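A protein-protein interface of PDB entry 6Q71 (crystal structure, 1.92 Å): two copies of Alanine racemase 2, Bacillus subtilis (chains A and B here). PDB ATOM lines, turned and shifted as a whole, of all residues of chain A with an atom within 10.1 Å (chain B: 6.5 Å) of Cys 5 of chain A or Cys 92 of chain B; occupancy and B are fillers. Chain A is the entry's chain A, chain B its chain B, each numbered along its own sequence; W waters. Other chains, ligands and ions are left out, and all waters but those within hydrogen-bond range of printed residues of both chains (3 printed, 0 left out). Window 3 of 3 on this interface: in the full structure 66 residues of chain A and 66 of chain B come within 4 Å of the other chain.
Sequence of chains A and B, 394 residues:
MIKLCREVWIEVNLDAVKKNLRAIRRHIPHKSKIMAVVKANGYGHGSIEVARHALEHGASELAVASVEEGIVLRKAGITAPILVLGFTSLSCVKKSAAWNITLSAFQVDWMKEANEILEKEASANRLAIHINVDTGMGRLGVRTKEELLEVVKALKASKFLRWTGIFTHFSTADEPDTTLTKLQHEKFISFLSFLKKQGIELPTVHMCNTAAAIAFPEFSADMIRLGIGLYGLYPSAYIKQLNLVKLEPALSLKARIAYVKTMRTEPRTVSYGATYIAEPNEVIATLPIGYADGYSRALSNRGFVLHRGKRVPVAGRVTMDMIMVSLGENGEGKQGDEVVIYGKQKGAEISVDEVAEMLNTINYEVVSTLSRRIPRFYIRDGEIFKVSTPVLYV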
ATOM      1  N   ILE A   2      20.623  13.247  30.840  1.00  0.00           N
ATOM      2  CA  ILE A   2      19.483  12.472  31.310  1.00  0.00           C
ATOM      3  C   ILE A   2      18.647  11.948  30.130  1.00  0.00           C
ATOM      4  O   ILE A   2      18.439  12.661  29.137  1.00  0.00           O
ATOM      5  CB  ILE A   2      18.610  13.353  32.270  1.00  0.00           C
ATOM      6  CG1 ILE A   2      19.350  13.609  33.590  1.00  0.00           C
ATOM      7  CG2 ILE A   2      17.296  12.688  32.592  1.00  0.00           C
ATOM      8  CD1 ILE A   2      19.444  15.061  33.964  1.00  0.00           C
ATOM      9  N   LYS A   3      18.193  10.701  30.234  1.00  0.00           N
ATOM     10  CA  LYS A   3      17.308  10.093  29.230  1.00  0.00           C
ATOM     11  C   LYS A   3      15.956   9.728  29.837  1.00  0.00           C
ATOM     12  O   LYS A   3      15.830   8.809  30.645  1.00  0.00           O
ATOM     13  CB  LYS A   3      17.948   8.845  28.589  1.00  0.00           C
ATOM     14  CG  LYS A   3      19.128   9.153  27.653  1.00  0.00           C
ATOM     15  CD  LYS A   3      19.542   7.930  26.823  1.00  0.00           C
ATOM     16  CE  LYS A   3      20.793   8.189  25.976  1.00  0.00           C
ATOM     17  NZ  LYS A   3      20.707   9.468  25.205  1.00  0.00           N
ATOM     18  N   LEU A   4      14.939  10.464  29.407  1.00  0.00           N
ATOM     19  CA  LEU A   4      13.592  10.313  29.914  1.00  0.00           C
ATOM     20  C   LEU A   4      12.621  10.202  28.753  1.00  0.00           C
ATOM     21  O   LEU A   4      12.858  10.745  27.664  1.00  0.00           O
ATOM     22  CB  LEU A   4      13.214  11.509  30.787  1.00  0.00           C
ATOM     23  CG  LEU A   4      14.049  11.708  32.055  1.00  0.00           C
ATOM     24  CD1 LEU A   4      13.904  13.130  32.532  1.00  0.00           C
ATOM     25  CD2 LEU A   4      13.620  10.731  33.143  1.00  0.00           C
ATOM     26  N   CYS A   5      11.496   9.549  29.004  1.00  0.00           N
ATOM     27  CA  CYS A   5      10.431   9.489  28.024  1.00  0.00           C
ATOM     28  C   CYS A   5       9.675  10.831  28.017  1.00  0.00           C
ATOM     29  O   CYS A   5       9.441  11.429  26.960  1.00  0.00           O
ATOM     30  CB  CYS A   5       9.476   8.339  28.342  1.00  0.00           C
ATOM     31  SG  CYS A   5      10.219   6.738  28.457  1.00  0.00           S
ATOM     32  N   ARG A   6       9.281  11.254  29.217  1.00  0.00           N
ATOM     33  CA  ARG A   6       8.650  12.534  29.465  1.00  0.00           C
ATOM     34  C   ARG A   6       9.721  13.390  30.092  1.00  0.00           C
ATOM     35  O   ARG A   6      10.212  13.049  31.174  1.00  0.00           O
ATOM     36  CB  ARG A   6       7.429  12.388  30.385  1.00  0.00           C
ATOM     37  CG  ARG A   6       6.647  13.700  30.563  1.00  0.00           C
ATOM     38  CD  ARG A   6       5.319  13.490  31.246  1.00  0.00           C
ATOM     39  NE  ARG A   6       4.604  14.748  31.477  1.00  0.00           N
ATOM     40  CZ  ARG A   6       4.438  15.329  32.668  1.00  0.00           C
ATOM     41  NH1 ARG A   6       4.924  14.788  33.787  1.00  0.00           N
ATOM     42  NH2 ARG A   6       3.739  16.445  32.753  1.00  0.00           N
ATOM     43  N   GLU A   7      10.130  14.452  29.405  1.00  0.00           N
ATOM     44  CA  GLU A   7      11.363  15.148  29.765  1.00  0.00           C
ATOM     45  C   GLU A   7      11.167  16.308  30.752  1.00  0.00           C
ATOM     46  O   GLU A   7      11.370  17.464  30.402  1.00  0.00           O
ATOM     47  CB  GLU A   7      12.038  15.638  28.496  1.00  0.00           C
ATOM     48  CG  GLU A   7      12.500  14.489  27.651  1.00  0.00           C
ATOM     49  CD  GLU A   7      13.086  14.910  26.312  1.00  0.00           C
ATOM     50  OE1 GLU A   7      14.238  14.501  26.051  1.00  0.00           O
ATOM     51  OE2 GLU A   7      12.391  15.610  25.531  1.00  0.00           O
ATOM     52  N   VAL A   8      10.742  15.966  31.971  1.00  0.00           N
ATOM     53  CA  VAL A   8      10.604  16.901  33.083  1.00  0.00           C
ATOM     54  C   VAL A   8      11.260  16.197  34.279  1.00  0.00           C
ATOM     55  O   VAL A   8      11.040  15.012  34.486  1.00  0.00           O
ATOM     56  CB  VAL A   8       9.117  17.273  33.368  1.00  0.00           C
ATOM     57  CG1 VAL A   8       8.271  16.013  33.682  1.00  0.00           C
ATOM     58  CG2 VAL A   8       8.994  18.272  34.483  1.00  0.00           C
ATOM     59  N   TRP A   9      12.071  16.901  35.057  1.00  0.00           N
ATOM     60  CA  TRP A   9      12.746  16.257  36.171  1.00  0.00           C
ATOM     61  C   TRP A   9      13.137  17.277  37.240  1.00  0.00           C
ATOM     62  O   TRP A   9      13.167  18.490  36.981  1.00  0.00           O
ATOM     63  CB  TRP A   9      13.986  15.478  35.675  1.00  0.00           C
ATOM     64  CG  TRP A   9      15.140  16.338  35.194  1.00  0.00           C
ATOM     65  CD1 TRP A   9      16.234  16.701  35.909  1.00  0.00           C
ATOM     66  CD2 TRP A   9      15.296  16.944  33.895  1.00  0.00           C
ATOM     67  NE1 TRP A   9      17.068  17.474  35.152  1.00  0.00           N
ATOM     68  CE2 TRP A   9      16.513  17.649  33.911  1.00  0.00           C
ATOM     69  CE3 TRP A   9      14.526  16.956  32.727  1.00  0.00           C
ATOM     70  CZ2 TRP A   9      16.986  18.366  32.799  1.00  0.00           C
ATOM     71  CZ3 TRP A   9      14.993  17.663  31.631  1.00  0.00           C
ATOM     72  CH2 TRP A   9      16.213  18.371  31.682  1.00  0.00           C
ATOM     73  N   ARG A 256      12.663  19.630  29.086  1.00  0.00           N
ATOM     74  CA  ARG A 256      13.111  19.922  27.738  1.00  0.00           C
ATOM     75  C   ARG A 256      11.953  20.244  26.820  1.00  0.00           C
ATOM     76  O   ARG A 256      10.857  19.677  26.941  1.00  0.00           O
ATOM     77  CB  ARG A 256      13.940  18.781  27.164  1.00  0.00           C
ATOM     78  CG  ARG A 256      15.306  18.717  27.839  1.00  0.00           C
ATOM     79  CD  ARG A 256      16.294  17.858  27.090  1.00  0.00           C
ATOM     80  NE  ARG A 256      16.129  16.454  27.335  1.00  0.00           N
ATOM     81  CZ  ARG A 256      16.847  15.747  28.207  1.00  0.00           C
ATOM     82  NH1 ARG A 256      17.793  16.301  28.939  1.00  0.00           N
ATOM     83  NH2 ARG A 256      16.598  14.460  28.343  1.00  0.00           N
ATOM     84  N   ILE A 257      12.205  21.163  25.897  1.00  0.00           N
ATOM     85  CA  ILE A 257      11.174  21.582  24.961  1.00  0.00           C
ATOM     86  C   ILE A 257      10.734  20.403  24.119  1.00  0.00           C
ATOM     87  O   ILE A 257      11.554  19.736  23.490  1.00  0.00           O
ATOM     88  CB  ILE A 257      11.649  22.708  24.038  1.00  0.00           C
ATOM     89  CG1 ILE A 257      12.007  23.940  24.869  1.00  0.00           C
ATOM     90  CG2 ILE A 257      10.556  23.024  23.010  1.00  0.00           C
ATOM     91  CD1 ILE A 257      12.356  25.196  24.047  1.00  0.00           C
ATOM     92  N   ALA A 258       9.425  20.167  24.112  1.00  0.00           N
ATOM     93  CA  ALA A 258       8.829  19.022  23.433  1.00  0.00           C
ATOM     94  C   ALA A 258       8.560  19.320  21.941  1.00  0.00           C
ATOM     95  O   ALA A 258       8.627  18.421  21.086  1.00  0.00           O
ATOM     96  CB  ALA A 258       7.541  18.651  24.117  1.00  0.00           C
ATOM     97  N   PRO A 288       6.655  19.757  28.808  1.00  0.00           N
ATOM     98  CA  PRO A 288       5.942  18.647  29.456  1.00  0.00           C
ATOM     99  C   PRO A 288       5.852  18.772  30.973  1.00  0.00           C
ATOM    100  O   PRO A 288       6.344  17.908  31.713  1.00  0.00           O
ATOM    101  CB  PRO A 288       6.777  17.441  29.049  1.00  0.00           C
ATOM    102  CG  PRO A 288       8.217  18.002  29.108  1.00  0.00           C
ATOM    103  CD  PRO A 288       8.049  19.385  28.478  1.00  0.00           C
ATOM    104  N   ARG A 373       5.318  11.837  40.321  1.00  0.00           N
ATOM    105  CA  ARG A 373       5.575  11.378  38.951  1.00  0.00           C
ATOM    106  C   ARG A 373       6.728  12.142  38.272  1.00  0.00           C
ATOM    107  O   ARG A 373       7.172  11.762  37.181  1.00  0.00           O
ATOM    108  CB  ARG A 373       4.291  11.447  38.095  1.00  0.00           C
ATOM    109  CG  ARG A 373       3.912  12.795  37.528  1.00  0.00           C
ATOM    110  CD  ARG A 373       2.799  12.630  36.446  1.00  0.00           C
ATOM    111  NE  ARG A 373       2.419  13.939  35.932  1.00  0.00           N
ATOM    112  CZ  ARG A 373       1.438  14.200  35.075  1.00  0.00           C
ATOM    113  NH1 ARG A 373       0.685  13.232  34.529  1.00  0.00           N
ATOM    114  NH2 ARG A 373       1.226  15.468  34.745  1.00  0.00           N
ATOM    115  N   PRO A 375      10.543  12.567  38.154  1.00  0.00           N
ATOM    116  CA  PRO A 375      11.704  11.864  38.711  1.00  0.00           C
ATOM    117  C   PRO A 375      12.697  12.845  39.322  1.00  0.00           C
ATOM    118  O   PRO A 375      12.874  13.940  38.801  1.00  0.00           O
ATOM    119  CB  PRO A 375      12.297  11.151  37.494  1.00  0.00           C
ATOM    120  CG  PRO A 375      11.867  11.979  36.321  1.00  0.00           C
ATOM    121  CD  PRO A 375      10.486  12.477  36.682  1.00  0.00           C
ATOM    122  N   PHE A 377      16.576  13.647  40.481  1.00  0.00           N
ATOM    123  CA  PHE A 377      18.007  13.362  40.377  1.00  0.00           C
ATOM    124  C   PHE A 377      18.778  14.133  41.433  1.00  0.00           C
ATOM    125  O   PHE A 377      18.408  15.257  41.777  1.00  0.00           O
ATOM    126  CB  PHE A 377      18.521  13.723  39.002  1.00  0.00           C
ATOM    127  CG  PHE A 377      17.877  12.941  37.906  1.00  0.00           C
ATOM    128  CD1 PHE A 377      16.643  13.307  37.401  1.00  0.00           C
ATOM    129  CD2 PHE A 377      18.513  11.837  37.376  1.00  0.00           C
ATOM    130  CE1 PHE A 377      16.050  12.570  36.392  1.00  0.00           C
ATOM    131  CE2 PHE A 377      17.922  11.098  36.364  1.00  0.00           C
ATOM    132  CZ  PHE A 377      16.691  11.471  35.869  1.00  0.00           C
ATOM    133  N   SER B  66       2.198   9.697  29.643  1.00  0.00           N
ATOM    134  CA  SER B  66       3.591   9.293  29.398  1.00  0.00           C
ATOM    135  C   SER B  66       3.727   7.784  29.256  1.00  0.00           C
ATOM    136  O   SER B  66       2.865   7.009  29.704  1.00  0.00           O
ATOM    137  CB  SER B  66       4.503   9.752  30.531  1.00  0.00           C
ATOM    138  OG  SER B  66       4.170   9.045  31.714  1.00  0.00           O
ATOM    139  N   VAL B  67       4.821   7.362  28.647  1.00  0.00           N
ATOM    140  CA  VAL B  67       5.116   5.936  28.576  1.00  0.00           C
ATOM    141  C   VAL B  67       5.156   5.339  29.982  1.00  0.00           C
ATOM    142  O   VAL B  67       4.631   4.241  30.213  1.00  0.00           O
ATOM    143  CB  VAL B  67       6.461   5.673  27.852  1.00  0.00           C
ATOM    144  CG1 VAL B  67       6.849   4.194  27.939  1.00  0.00           C
ATOM    145  CG2 VAL B  67       6.341   6.067  26.413  1.00  0.00           C
ATOM    146  N   GLU B  68       5.767   6.051  30.933  1.00  0.00           N
ATOM    147  CA  GLU B  68       5.915   5.473  32.261  1.00  0.00           C
ATOM    148  C   GLU B  68       4.493   5.138  32.828  1.00  0.00           C
ATOM    149  O   GLU B  68       4.290   4.087  33.430  1.00  0.00           O
ATOM    150  CB  GLU B  68       6.709   6.418  33.190  1.00  0.00           C
ATOM    151  CG  GLU B  68       8.182   6.803  32.736  1.00  0.00           C
ATOM    152  CD  GLU B  68       8.296   8.142  31.899  1.00  0.00           C
ATOM    153  OE1 GLU B  68       9.317   8.905  32.005  1.00  0.00           O
ATOM    154  OE2 GLU B  68       7.371   8.423  31.114  1.00  0.00           O
ATOM    155  N   ILE B  71       3.254   1.947  31.190  1.00  0.00           N
ATOM    156  CA  ILE B  71       3.935   0.756  31.689  1.00  0.00           C
ATOM    157  C   ILE B  71       3.371   0.318  33.061  1.00  0.00           C
ATOM    158  O   ILE B  71       3.237  -0.880  33.333  1.00  0.00           O
ATOM    159  CB  ILE B  71       5.439   0.993  31.760  1.00  0.00           C
ATOM    160  CG1 ILE B  71       5.994   1.038  30.334  1.00  0.00           C
ATOM    161  CG2 ILE B  71       6.143  -0.108  32.574  1.00  0.00           C
ATOM    162  CD1 ILE B  71       7.484   1.294  30.267  1.00  0.00           C
ATOM    163  N   PHE B  87       4.158  14.302  24.267  1.00  0.00           N
ATOM    164  CA  PHE B  87       5.331  14.003  23.470  1.00  0.00           C
ATOM    165  C   PHE B  87       6.202  12.944  24.153  1.00  0.00           C
ATOM    166  O   PHE B  87       6.506  13.024  25.356  1.00  0.00           O
ATOM    167  CB  PHE B  87       6.155  15.282  23.222  1.00  0.00           C
ATOM    168  CG  PHE B  87       7.482  15.025  22.551  1.00  0.00           C
ATOM    169  CD1 PHE B  87       7.538  14.792  21.188  1.00  0.00           C
ATOM    170  CD2 PHE B  87       8.675  15.016  23.291  1.00  0.00           C
ATOM    171  CE1 PHE B  87       8.740  14.557  20.544  1.00  0.00           C
ATOM    172  CE2 PHE B  87       9.894  14.782  22.669  1.00  0.00           C
ATOM    173  CZ  PHE B  87       9.935  14.544  21.292  1.00  0.00           C
ATOM    174  N   THR B  88       6.616  11.967  23.361  1.00  0.00           N
ATOM    175  CA  THR B  88       7.552  10.950  23.821  1.00  0.00           C
ATOM    176  C   THR B  88       8.875  11.075  23.092  1.00  0.00           C
ATOM    177  O   THR B  88       8.949  11.018  21.862  1.00  0.00           O
ATOM    178  CB  THR B  88       6.974   9.545  23.636  1.00  0.00           C
ATOM    179  OG1 THR B  88       5.798   9.433  24.460  1.00  0.00           O
ATOM    180  CG2 THR B  88       7.988   8.501  24.032  1.00  0.00           C
ATOM    181  N   SER B  89       9.924  11.241  23.888  1.00  0.00           N
ATOM    182  CA  SER B  89      11.266  11.310  23.367  1.00  0.00           C
ATOM    183  C   SER B  89      11.649  10.015  22.619  1.00  0.00           C
ATOM    184  O   SER B  89      11.243   8.902  22.970  1.00  0.00           O
ATOM    185  CB  SER B  89      12.238  11.604  24.509  1.00  0.00           C
ATOM    186  OG  SER B  89      13.530  11.113  24.211  1.00  0.00           O
ATOM    187  N   LEU B  90      12.440  10.172  21.570  1.00  0.00           N
ATOM    188  CA  LEU B  90      12.907   9.036  20.785  1.00  0.00           C
ATOM    189  C   LEU B  90      13.700   8.031  21.637  1.00  0.00           C
ATOM    190  O   LEU B  90      13.795   6.842  21.300  1.00  0.00           O
ATOM    191  CB  LEU B  90      13.746   9.531  19.598  1.00  0.00           C
ATOM    192  CG  LEU B  90      12.912  10.208  18.502  1.00  0.00           C
ATOM    193  CD1 LEU B  90      13.784  10.972  17.510  1.00  0.00           C
ATOM    194  CD2 LEU B  90      12.084   9.177  17.763  1.00  0.00           C
ATOM    195  N   SER B  91      14.209   8.493  22.775  1.00  0.00           N
ATOM    196  CA  SER B  91      14.931   7.606  23.685  1.00  0.00           C
ATOM    197  C   SER B  91      14.053   6.466  24.213  1.00  0.00           C
ATOM    198  O   SER B  91      14.564   5.476  24.710  1.00  0.00           O
ATOM    199  CB  SER B  91      15.451   8.403  24.879  1.00  0.00           C
ATOM    200  OG  SER B  91      16.333   9.418  24.459  1.00  0.00           O
ATOM    201  N   CYS B  92      12.738   6.606  24.119  1.00  0.00           N
ATOM    202  CA  CYS B  92      11.821   5.587  24.638  1.00  0.00           C
ATOM    203  C   CYS B  92      11.063   4.821  23.568  1.00  0.00           C
ATOM    204  O   CYS B  92      10.146   4.114  23.880  1.00  0.00           O
ATOM    205  CB  CYS B  92      10.797   6.176  25.649  1.00  0.00           C
ATOM    206  SG  CYS B  92      11.512   6.766  27.137  1.00  0.00           S
ATOM    207  N   VAL B  93      11.458   4.945  22.326  1.00  0.00           N
ATOM    208  CA  VAL B  93      10.730   4.244  21.260  1.00  0.00           C
ATOM    209  C   VAL B  93      10.861   2.724  21.427  1.00  0.00           C
ATOM    210  O   VAL B  93       9.866   1.990  21.396  1.00  0.00           O
ATOM    211  CB  VAL B  93      11.232   4.733  19.883  1.00  0.00           C
ATOM    212  CG1 VAL B  93      11.113   3.662  18.802  1.00  0.00           C
ATOM    213  CG2 VAL B  93      10.477   6.019  19.512  1.00  0.00           C
ATOM    214  N   LYS B  94      12.085   2.261  21.665  1.00  0.00           N
ATOM    215  CA  LYS B  94      12.355   0.841  21.861  1.00  0.00           C
ATOM    216  C   LYS B  94      11.493   0.212  22.938  1.00  0.00           C
ATOM    217  O   LYS B  94      10.775  -0.759  22.714  1.00  0.00           O
ATOM    218  CB  LYS B  94      13.813   0.670  22.250  1.00  0.00           C
ATOM    219  CG  LYS B  94      14.261  -0.736  22.554  1.00  0.00           C
ATOM    220  CD  LYS B  94      15.761  -0.687  22.837  1.00  0.00           C
ATOM    221  CE  LYS B  94      16.224  -1.818  23.710  1.00  0.00           C
ATOM    222  NZ  LYS B  94      16.265  -3.105  23.009  1.00  0.00           N
ATOM    223  N   LYS B  95      11.566   0.823  24.104  1.00  0.00           N
ATOM    224  CA  LYS B  95      10.761   0.490  25.254  1.00  0.00           C
ATOM    225  C   LYS B  95       9.245   0.519  24.968  1.00  0.00           C
ATOM    226  O   LYS B  95       8.502  -0.363  25.434  1.00  0.00           O
ATOM    227  CB  LYS B  95      11.086   1.492  26.344  1.00  0.00           C
ATOM    228  CG  LYS B  95      10.477   1.264  27.693  1.00  0.00           C
ATOM    229  CD  LYS B  95      10.585   2.560  28.493  1.00  0.00           C
ATOM    230  CE  LYS B  95      11.981   2.874  28.921  1.00  0.00           C
ATOM    231  NZ  LYS B  95      12.168   2.655  30.366  1.00  0.00           N
ATOM    232  N   SER B  96       8.771   1.547  24.251  1.00  0.00           N
ATOM    233  CA  SER B  96       7.313   1.673  24.019  1.00  0.00           C
ATOM    234  C   SER B  96       6.845   0.554  23.128  1.00  0.00           C
ATOM    235  O   SER B  96       5.791  -0.010  23.338  1.00  0.00           O
ATOM    236  CB  SER B  96       6.953   3.017  23.377  1.00  0.00           C
ATOM    237  OG  SER B  96       7.387   4.109  24.170  1.00  0.00           O
ATOM    238  N   ALA B  97       7.668   0.218  22.139  1.00  0.00           N
ATOM    239  CA  ALA B  97       7.370  -0.871  21.219  1.00  0.00           C
ATOM    240  C   ALA B  97       7.323  -2.221  21.961  1.00  0.00           C
ATOM    241  O   ALA B  97       6.388  -3.010  21.775  1.00  0.00           O
ATOM    242  CB  ALA B  97       8.405  -0.905  20.115  1.00  0.00           C
ATOM    243  N   LEU B 103       2.112   5.564  20.779  1.00  0.00           N
ATOM    244  CA  LEU B 103       2.613   6.908  20.954  1.00  0.00           C
ATOM    245  C   LEU B 103       1.941   7.838  19.955  1.00  0.00           C
ATOM    246  O   LEU B 103       1.651   7.468  18.813  1.00  0.00           O
ATOM    247  CB  LEU B 103       4.148   6.970  20.777  1.00  0.00           C
ATOM    248  CG  LEU B 103       4.948   6.022  21.688  1.00  0.00           C
ATOM    249  CD1 LEU B 103       6.438   6.151  21.400  1.00  0.00           C
ATOM    250  CD2 LEU B 103       4.635   6.282  23.153  1.00  0.00           C
ATOM    251  N   LEU B 127       5.838  -0.415  16.464  1.00  0.00           N
ATOM    252  CA  LEU B 127       5.336   0.642  17.310  1.00  0.00           C
ATOM    253  C   LEU B 127       4.031   1.267  16.737  1.00  0.00           C
ATOM    254  O   LEU B 127       3.998   1.758  15.605  1.00  0.00           O
ATOM    255  CB  LEU B 127       6.433   1.692  17.467  1.00  0.00           C
ATOM    256  CG  LEU B 127       6.105   2.925  18.321  1.00  0.00           C
ATOM    257  CD1 LEU B 127       5.881   2.555  19.802  1.00  0.00           C
ATOM    258  CD2 LEU B 127       7.227   3.899  18.131  1.00  0.00           C
HETATM  259  O   HOH W   1      14.639   7.248  28.110  1.00  0.00           O
HETATM  260  O   HOH W   2      15.548  11.818  26.822  1.00  0.00           O
HETATM  261  O   HOH W   3       8.526  14.895  27.283  1.00  0.00           O
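N of Ser 89 of chain B lies within hydrogen-bond range of O of Cys 5 of chain A, 3.1 Å away. SG of Cys 5 of chain A is disulfide-bonded to SG of Cys 92 of chain B.
The backbone carbonyl oxygen of Pro 288 of chain A is in hydrogen-bond range of the guanidinium group of Arg 6 of chain A, 3.2 Å away. The side-chain carboxylate (OE1) of Glu 7 of chain A is in salt-bridge range of the guanidinium group (NE) of Arg 256 of chain A (3.0 Å). The side-chain carboxylate of Glu 68 of chain B sits close to the side-chain hydroxyl of Ser 66 of chain B, at 3.3 Å. OG of Ser 89 of chain B sits close to N of Ser 91 of chain B (3.1 Å). The side-chain hydroxyl (OG) of Ser 96 of chain B is in hydrogen-bond range of the backbone carbonyl oxygen (O) of Cys 92 of chain B (2.8 Å).
SG of Cys 92 of chain B touches C of Leu 4 of chain A, 3.96 Å away. Cys 5 of chain A touches Val 67 of chain B. OE2 of Glu 68 of chain B touches CB of Cys 5 of chain A (3.5 Å). Phe 87 of chain B touches Cys 5 of chain A. Cys 5 of chain A touches Thr 88 of chain B (O to CA, 3.7 Å). Arg 6 of chain A touches Ser 66 of chain B (CD to CB, 3.9 Å). N of Arg 6 of chain A touches OE1 of Glu 68 of chain B, 3.6 Å away. Glu 7 of chain A touches Phe 87 of chain B (OE2 to CE2, 3.9 Å). Ser 89 of chain B touches Glu 7 of chain A. Ala 258 of chain A touches Phe 87 of chain B (CB to CB, 3.8 Å).
Of chain B, only Val 67 (3.95 Å), Glu 68 (3.5 Å), Phe 87 (3.7 Å), Thr 88 (3.7 Å), Ser 89 (3.1 Å) and Cys 92 (1.8 Å) come within 4 Å of Cys 5 of chain A. Cys 92 of chain B touches two residues of chain A. Of chain A, only Cys 5 (3.7 Å) comes within 4 Å of Thr 88 of chain B. No residue of chain A comes within 4 Å of Ser 91 of chain B. No residue of chain A comes within 4 Å of Val 93 of chain B. No residue of chain A comes within 4 Å of Lys 95 of chain B. Printed residues of chain A within 4 Å of Glu 68 of chain B: Cys 5 (3.5 Å) and Arg 6 (3.6 Å). Printed residues of chain A within 4 Å of Val 67 of chain B: Cys 5. Phe 377 of chain A touches none of the printed residues of chain B. Ile 257 of chain A touches none of the printed residues of chain B. The nearest residue of chain A that does not touch Cys 92 of chain B is Arg 6 of chain A (5.4 Å). The nearest printed residue of chain A that does not touch Val 67 of chain B is Arg 6 of chain A (5.9 Å).
Hydrophobic or aromatic side chains of chain A within 4 Å of the printed part of chain B: Ala 258. Along chain A the printed residues that touch a printed residue of chain B span positions 4 to 258. Hydrophobic or aromatic side chains of chain B within 4 Å of the printed part of chain A: Val 67 and Phe 87. Along chain B the printed residues that touch a printed residue of chain A span positions 66 to 92. Among the printed residues, 13 pairs touch across the chains.
No position is printed for both chains.
Water W3 bridges N of Glu 7 of chain A (2.7 Å) and O of Phe 87 of chain B (3.4 Å). Water W2 lies within hydrogen-bond range of N of Leu 4 of chain A, OE1 of Glu 7 of chain A, NH2 of Arg 256 of chain A, OG of Ser 89 of chain B and OG of Ser 91 of chain B. Water W1 lies within hydrogen-bond range of the backbone carbonyl oxygen (O) of Lys 3 of chain A, the side-chain sulfur (SG) of Cys 92 of chain B and the backbone NH (N) of Leu 4 of chain A.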
